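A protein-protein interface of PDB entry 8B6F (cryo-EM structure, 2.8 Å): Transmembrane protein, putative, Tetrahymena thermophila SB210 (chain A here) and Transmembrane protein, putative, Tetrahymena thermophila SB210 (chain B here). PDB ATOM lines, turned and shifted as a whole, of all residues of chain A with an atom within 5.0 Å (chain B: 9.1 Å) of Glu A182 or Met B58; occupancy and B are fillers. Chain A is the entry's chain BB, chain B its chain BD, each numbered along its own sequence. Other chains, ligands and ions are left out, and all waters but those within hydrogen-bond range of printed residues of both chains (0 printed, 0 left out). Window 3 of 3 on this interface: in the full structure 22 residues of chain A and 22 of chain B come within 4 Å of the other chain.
OE1 of Glu A183 is in salt-bridge range of NZ of Lys B159.
N of Met B58 lies within hydrogen-bond range of OE1 of Glu A182.
Phe A175 touches Met B58.
Thr A179 touches Lys B159 (CG2 to NZ, 3.4 Å).
Ala A180 touches Leu B156 (O to CD1, 3.8 Å).
CB of Leu B156 touches CD of Glu A183 (3.7 Å).
Ile A184 touches Leu B156 (CG1 to CD1, 3.8 Å).
Ile A184 touches Trp B170 (CG2 to CZ3, 3.9 Å).
Of the printed residues of chain B, Ala A180 touches Leu B156.
No residue of chain B comes within 4 Å of Ala A181.
Glu A182 touches just one residue of chain B: Met B58.
Met B58 touches just these residues of chain A: Phe A175 and Glu A182.
Glu B148 touches none of the printed residues of chain A.
Of the printed residues of chain A, Leu B156 touches Ala A180, Glu A183 and Ile A184.
Printed residues of chain A within 4 Å of Lys B159: Thr A179 and Glu A183.
The nearest residue of chain B that does not touch Glu A182 is Gln B59 (6.3 Å).
The nearest printed residue of chain B that does not touch Ala A180 is Lys B159 (4.1 Å).
Of the 11 printed residues of chain A, 6 touch a printed residue of chain B.
Hydrophobic or aromatic side chains of chain A that line the printed part of chain B: Phe A175 and Ile A184.
Hydrophobic or aromatic side chains of chain B within 4 Å of the printed part of chain A: Met B58, Leu B156 and Trp B170.
Among the printed residues, Asp or Glu carboxylates within 4 Å of a Lys or Arg side-chain nitrogen of the other chain: Glu A183 with Lys B159 (2.8 Å).
The side-chain hydroxyl of Thr A179 lies within hydrogen-bond range of the backbone carbonyl oxygen of Phe A175, 2.9 Å away.
OD1 of Asn A178 lies close to OE2 of Glu A182 (3.1 Å).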
ATOM      1  N   PHE A 175     -39.429 -20.484   2.888  1.00  0.00           N
ATOM      2  CA  PHE A 175     -38.593 -19.413   2.356  1.00  0.00           C
ATOM      3  C   PHE A 175     -37.115 -19.699   2.594  1.00  0.00           C
ATOM      4  O   PHE A 175     -36.287 -19.547   1.688  1.00  0.00           O
ATOM      5  CB  PHE A 175     -38.994 -18.078   2.989  1.00  0.00           C
ATOM      6  CG  PHE A 175     -38.295 -16.891   2.392  1.00  0.00           C
ATOM      7  CD1 PHE A 175     -37.078 -16.458   2.889  1.00  0.00           C
ATOM      8  CD2 PHE A 175     -38.862 -16.205   1.333  1.00  0.00           C
ATOM      9  CE1 PHE A 175     -36.439 -15.365   2.337  1.00  0.00           C
ATOM     10  CE2 PHE A 175     -38.230 -15.114   0.778  1.00  0.00           C
ATOM     11  CZ  PHE A 175     -37.018 -14.692   1.280  1.00  0.00           C
ATOM     12  N   ASN A 178     -35.949 -22.576   0.362  1.00  0.00           N
ATOM     13  CA  ASN A 178     -35.819 -22.138  -1.023  1.00  0.00           C
ATOM     14  C   ASN A 178     -34.564 -21.299  -1.218  1.00  0.00           C
ATOM     15  O   ASN A 178     -33.877 -21.430  -2.238  1.00  0.00           O
ATOM     16  CB  ASN A 178     -37.060 -21.357  -1.447  1.00  0.00           C
ATOM     17  CG  ASN A 178     -36.954 -20.827  -2.862  1.00  0.00           C
ATOM     18  OD1 ASN A 178     -36.635 -19.660  -3.076  1.00  0.00           O
ATOM     19  ND2 ASN A 178     -37.210 -21.690  -3.838  1.00  0.00           N
ATOM     20  N   THR A 179     -34.248 -20.431  -0.258  1.00  0.00           N
ATOM     21  CA  THR A 179     -33.006 -19.672  -0.342  1.00  0.00           C
ATOM     22  C   THR A 179     -31.804 -20.608  -0.355  1.00  0.00           C
ATOM     23  O   THR A 179     -30.865 -20.416  -1.135  1.00  0.00           O
ATOM     24  CB  THR A 179     -32.905 -18.694   0.829  1.00  0.00           C
ATOM     25  OG1 THR A 179     -34.092 -17.894   0.892  1.00  0.00           O
ATOM     26  CG2 THR A 179     -31.698 -17.785   0.667  1.00  0.00           C
ATOM     27  N   ALA A 180     -31.818 -21.625   0.506  1.00  0.00           N
ATOM     28  CA  ALA A 180     -30.726 -22.592   0.529  1.00  0.00           C
ATOM     29  C   ALA A 180     -30.615 -23.327  -0.800  1.00  0.00           C
ATOM     30  O   ALA A 180     -29.509 -23.557  -1.300  1.00  0.00           O
ATOM     31  CB  ALA A 180     -30.929 -23.582   1.675  1.00  0.00           C
ATOM     32  N   ALA A 181     -31.751 -23.708  -1.384  1.00  0.00           N
ATOM     33  CA  ALA A 181     -31.726 -24.404  -2.666  1.00  0.00           C
ATOM     34  C   ALA A 181     -31.142 -23.526  -3.763  1.00  0.00           C
ATOM     35  O   ALA A 181     -30.358 -23.996  -4.595  1.00  0.00           O
ATOM     36  CB  ALA A 181     -33.136 -24.859  -3.040  1.00  0.00           C
ATOM     37  N   GLU A 182     -31.522 -22.248  -3.792  1.00  0.00           N
ATOM     38  CA  GLU A 182     -30.971 -21.339  -4.789  1.00  0.00           C
ATOM     39  C   GLU A 182     -29.468 -21.170  -4.612  1.00  0.00           C
ATOM     40  O   GLU A 182     -28.721 -21.133  -5.596  1.00  0.00           O
ATOM     41  CB  GLU A 182     -31.681 -19.988  -4.709  1.00  0.00           C
ATOM     42  CG  GLU A 182     -33.136 -20.048  -5.140  1.00  0.00           C
ATOM     43  CD  GLU A 182     -33.857 -18.728  -4.953  1.00  0.00           C
ATOM     44  OE1 GLU A 182     -33.287 -17.825  -4.304  1.00  0.00           O
ATOM     45  OE2 GLU A 182     -34.991 -18.595  -5.456  1.00  0.00           O
ATOM     46  N   GLU A 183     -29.006 -21.067  -3.365  1.00  0.00           N
ATOM     47  CA  GLU A 183     -27.572 -20.959  -3.122  1.00  0.00           C
ATOM     48  C   GLU A 183     -26.844 -22.216  -3.580  1.00  0.00           C
ATOM     49  O   GLU A 183     -25.749 -22.136  -4.147  1.00  0.00           O
ATOM     50  CB  GLU A 183     -27.310 -20.687  -1.641  1.00  0.00           C
ATOM     51  CG  GLU A 183     -25.891 -20.230  -1.351  1.00  0.00           C
ATOM     52  CD  GLU A 183     -25.763 -19.547  -0.004  1.00  0.00           C
ATOM     53  OE1 GLU A 183     -26.776 -19.469   0.723  1.00  0.00           O
ATOM     54  OE2 GLU A 183     -24.652 -19.083   0.326  1.00  0.00           O
ATOM     55  N   ILE A 184     -27.432 -23.388  -3.335  1.00  0.00           N
ATOM     56  CA  ILE A 184     -26.834 -24.633  -3.806  1.00  0.00           C
ATOM     57  C   ILE A 184     -26.736 -24.628  -5.324  1.00  0.00           C
ATOM     58  O   ILE A 184     -25.721 -25.043  -5.897  1.00  0.00           O
ATOM     59  CB  ILE A 184     -27.639 -25.841  -3.291  1.00  0.00           C
ATOM     60  CG1 ILE A 184     -27.430 -26.005  -1.784  1.00  0.00           C
ATOM     61  CG2 ILE A 184     -27.245 -27.119  -4.035  1.00  0.00           C
ATOM     62  CD1 ILE A 184     -28.313 -27.056  -1.146  1.00  0.00           C
ATOM     63  N   GLU A 185     -27.783 -24.158  -6.002  1.00  0.00           N
ATOM     64  CA  GLU A 185     -27.751 -24.102  -7.459  1.00  0.00           C
ATOM     65  C   GLU A 185     -26.659 -23.161  -7.952  1.00  0.00           C
ATOM     66  O   GLU A 185     -25.964 -23.465  -8.927  1.00  0.00           O
ATOM     67  CB  GLU A 185     -29.117 -23.685  -7.999  1.00  0.00           C
ATOM     68  CG  GLU A 185     -30.172 -24.770  -7.857  1.00  0.00           C
ATOM     69  CD  GLU A 185     -31.483 -24.410  -8.524  1.00  0.00           C
ATOM     70  OE1 GLU A 185     -31.656 -23.233  -8.905  1.00  0.00           O
ATOM     71  OE2 GLU A 185     -32.339 -25.306  -8.672  1.00  0.00           O
ATOM     72  N   ASP A 186     -26.486 -22.016  -7.290  1.00  0.00           N
ATOM     73  CA  ASP A 186     -25.406 -21.111  -7.672  1.00  0.00           C
ATOM     74  C   ASP A 186     -24.048 -21.779  -7.509  1.00  0.00           C
ATOM     75  O   ASP A 186     -23.179 -21.657  -8.380  1.00  0.00           O
ATOM     76  CB  ASP A 186     -25.471 -19.831  -6.840  1.00  0.00           C
ATOM     77  CG  ASP A 186     -26.711 -19.010  -7.128  1.00  0.00           C
ATOM     78  OD1 ASP A 186     -27.189 -19.041  -8.282  1.00  0.00           O
ATOM     79  OD2 ASP A 186     -27.207 -18.331  -6.204  1.00  0.00           O
ATOM     80  N   ARG A 189     -23.496 -24.087 -10.327  1.00  0.00           N
ATOM     81  CA  ARG A 189     -23.083 -23.370 -11.529  1.00  0.00           C
ATOM     82  C   ARG A 189     -21.595 -23.053 -11.490  1.00  0.00           C
ATOM     83  O   ARG A 189     -20.891 -23.219 -12.493  1.00  0.00           O
ATOM     84  CB  ARG A 189     -23.890 -22.082 -11.684  1.00  0.00           C
ATOM     85  CG  ARG A 189     -25.368 -22.294 -11.944  1.00  0.00           C
ATOM     86  CD  ARG A 189     -26.060 -20.974 -12.242  1.00  0.00           C
ATOM     87  NE  ARG A 189     -27.509 -21.121 -12.305  1.00  0.00           N
ATOM     88  CZ  ARG A 189     -28.334 -20.933 -11.282  1.00  0.00           C
ATOM     89  NH1 ARG A 189     -27.888 -20.578 -10.088  1.00  0.00           N
ATOM     90  NH2 ARG A 189     -29.640 -21.106 -11.461  1.00  0.00           N
ATOM     91  N   MET B  58     -33.258 -14.742  -2.841  1.00  0.00           N
ATOM     92  CA  MET B  58     -32.537 -13.484  -2.502  1.00  0.00           C
ATOM     93  C   MET B  58     -31.539 -13.121  -3.595  1.00  0.00           C
ATOM     94  O   MET B  58     -30.854 -13.988  -4.132  1.00  0.00           O
ATOM     95  CB  MET B  58     -31.814 -13.625  -1.161  1.00  0.00           C
ATOM     96  CG  MET B  58     -32.736 -13.624   0.052  1.00  0.00           C
ATOM     97  SD  MET B  58     -33.586 -12.051   0.285  1.00  0.00           S
ATOM     98  CE  MET B  58     -34.266 -12.271   1.926  1.00  0.00           C
ATOM     99  N   GLN B  59     -31.462 -11.832  -3.917  1.00  0.00           N
ATOM    100  CA  GLN B  59     -30.533 -11.345  -4.924  1.00  0.00           C
ATOM    101  C   GLN B  59     -30.114  -9.930  -4.560  1.00  0.00           C
ATOM    102  O   GLN B  59     -30.815  -9.225  -3.831  1.00  0.00           O
ATOM    103  CB  GLN B  59     -31.151 -11.378  -6.326  1.00  0.00           C
ATOM    104  CG  GLN B  59     -32.425 -10.557  -6.461  1.00  0.00           C
ATOM    105  CD  GLN B  59     -33.000 -10.609  -7.860  1.00  0.00           C
ATOM    106  OE1 GLN B  59     -32.428 -11.231  -8.753  1.00  0.00           O
ATOM    107  NE2 GLN B  59     -34.137  -9.956  -8.057  1.00  0.00           N
ATOM    108  N   ASN B  60     -28.960  -9.518  -5.080  1.00  0.00           N
ATOM    109  CA  ASN B  60     -28.440  -8.192  -4.774  1.00  0.00           C
ATOM    110  C   ASN B  60     -29.423  -7.115  -5.212  1.00  0.00           C
ATOM    111  O   ASN B  60     -29.950  -7.152  -6.327  1.00  0.00           O
ATOM    112  CB  ASN B  60     -27.090  -7.986  -5.460  1.00  0.00           C
ATOM    113  CG  ASN B  60     -25.996  -8.844  -4.859  1.00  0.00           C
ATOM    114  OD1 ASN B  60     -26.020  -9.155  -3.669  1.00  0.00           O
ATOM    115  ND2 ASN B  60     -25.027  -9.229  -5.681  1.00  0.00           N
ATOM    116  N   ALA B  61     -29.665  -6.152  -4.325  1.00  0.00           N
ATOM    117  CA  ALA B  61     -30.597  -5.062  -4.583  1.00  0.00           C
ATOM    118  C   ALA B  61     -29.912  -3.788  -5.059  1.00  0.00           C
ATOM    119  O   ALA B  61     -30.418  -3.121  -5.964  1.00  0.00           O
ATOM    120  CB  ALA B  61     -31.406  -4.757  -3.319  1.00  0.00           C
ATOM    121  N   GLU B 148     -32.840 -13.307  10.039  1.00  0.00           N
ATOM    122  CA  GLU B 148     -31.786 -12.404   9.584  1.00  0.00           C
ATOM    123  C   GLU B 148     -32.189 -10.971   9.917  1.00  0.00           C
ATOM    124  O   GLU B 148     -32.801 -10.273   9.110  1.00  0.00           O
ATOM    125  CB  GLU B 148     -31.530 -12.581   8.092  1.00  0.00           C
ATOM    126  CG  GLU B 148     -30.897 -13.914   7.737  1.00  0.00           C
ATOM    127  CD  GLU B 148     -30.690 -14.084   6.246  1.00  0.00           C
ATOM    128  OE1 GLU B 148     -31.051 -13.161   5.488  1.00  0.00           O
ATOM    129  OE2 GLU B 148     -30.169 -15.140   5.832  1.00  0.00           O
ATOM    130  N   ARG B 153     -25.476 -12.291   7.267  1.00  0.00           N
ATOM    131  CA  ARG B 153     -26.444 -13.178   6.643  1.00  0.00           C
ATOM    132  C   ARG B 153     -26.133 -14.629   6.982  1.00  0.00           C
ATOM    133  O   ARG B 153     -24.973 -15.028   7.102  1.00  0.00           O
ATOM    134  CB  ARG B 153     -26.443 -13.002   5.122  1.00  0.00           C
ATOM    135  CG  ARG B 153     -26.913 -11.642   4.640  1.00  0.00           C
ATOM    136  CD  ARG B 153     -28.348 -11.370   5.051  1.00  0.00           C
ATOM    137  NE  ARG B 153     -28.848 -10.121   4.488  1.00  0.00           N
ATOM    138  CZ  ARG B 153     -29.467 -10.012   3.321  1.00  0.00           C
ATOM    139  NH1 ARG B 153     -29.678 -11.063   2.548  1.00  0.00           N
ATOM    140  NH2 ARG B 153     -29.885  -8.816   2.920  1.00  0.00           N
ATOM    141  N   LYS B 154     -27.190 -15.421   7.131  1.00  0.00           N
ATOM    142  CA  LYS B 154     -27.021 -16.846   7.368  1.00  0.00           C
ATOM    143  C   LYS B 154     -26.408 -17.500   6.137  1.00  0.00           C
ATOM    144  O   LYS B 154     -26.876 -17.295   5.013  1.00  0.00           O
ATOM    145  CB  LYS B 154     -28.365 -17.490   7.703  1.00  0.00           C
ATOM    146  CG  LYS B 154     -29.059 -16.887   8.916  1.00  0.00           C
ATOM    147  CD  LYS B 154     -28.267 -17.117  10.193  1.00  0.00           C
ATOM    148  CE  LYS B 154     -28.986 -16.540  11.401  1.00  0.00           C
ATOM    149  NZ  LYS B 154     -28.252 -16.818  12.667  1.00  0.00           N
ATOM    150  N   LEU B 156     -24.807 -20.822   3.776  1.00  0.00           N
ATOM    151  CA  LEU B 156     -25.357 -22.090   3.313  1.00  0.00           C
ATOM    152  C   LEU B 156     -25.169 -23.182   4.357  1.00  0.00           C
ATOM    153  O   LEU B 156     -26.064 -24.008   4.568  1.00  0.00           O
ATOM    154  CB  LEU B 156     -24.707 -22.497   1.991  1.00  0.00           C
ATOM    155  CG  LEU B 156     -25.187 -23.825   1.403  1.00  0.00           C
ATOM    156  CD1 LEU B 156     -26.688 -23.810   1.171  1.00  0.00           C
ATOM    157  CD2 LEU B 156     -24.451 -24.132   0.113  1.00  0.00           C
ATOM    158  N   LYS B 159     -27.756 -22.667   7.099  1.00  0.00           N
ATOM    159  CA  LYS B 159     -29.080 -23.074   6.643  1.00  0.00           C
ATOM    160  C   LYS B 159     -29.179 -24.590   6.524  1.00  0.00           C
ATOM    161  O   LYS B 159     -30.227 -25.174   6.822  1.00  0.00           O
ATOM    162  CB  LYS B 159     -29.414 -22.398   5.314  1.00  0.00           C
ATOM    163  CG  LYS B 159     -29.967 -20.989   5.482  1.00  0.00           C
ATOM    164  CD  LYS B 159     -30.141 -20.276   4.153  1.00  0.00           C
ATOM    165  CE  LYS B 159     -28.808 -19.816   3.594  1.00  0.00           C
ATOM    166  NZ  LYS B 159     -28.975 -18.978   2.374  1.00  0.00           N
ATOM    167  N   TRP B 170     -24.579 -33.032   0.233  1.00  0.00           N
ATOM    168  CA  TRP B 170     -23.755 -31.973  -0.341  1.00  0.00           C
ATOM    169  C   TRP B 170     -22.291 -32.134   0.052  1.00  0.00           C
ATOM    170  O   TRP B 170     -21.396 -31.903  -0.768  1.00  0.00           O
ATOM    171  CB  TRP B 170     -24.296 -30.612   0.099  1.00  0.00           C
ATOM    172  CG  TRP B 170     -23.534 -29.438  -0.425  1.00  0.00           C
ATOM    173  CD1 TRP B 170     -22.773 -28.572   0.301  1.00  0.00           C
ATOM    174  CD2 TRP B 170     -23.459 -28.996  -1.785  1.00  0.00           C
ATOM    175  NE1 TRP B 170     -22.229 -27.618  -0.523  1.00  0.00           N
ATOM    176  CE2 TRP B 170     -22.635 -27.857  -1.808  1.00  0.00           C
ATOM    177  CE3 TRP B 170     -24.011 -29.453  -2.986  1.00  0.00           C
ATOM    178  CZ2 TRP B 170     -22.348 -27.167  -2.984  1.00  0.00           C
ATOM    179  CZ3 TRP B 170     -23.726 -28.768  -4.153  1.00  0.00           C
ATOM    180  CH2 TRP B 170     -22.900 -27.637  -4.144  1.00  0.00           C
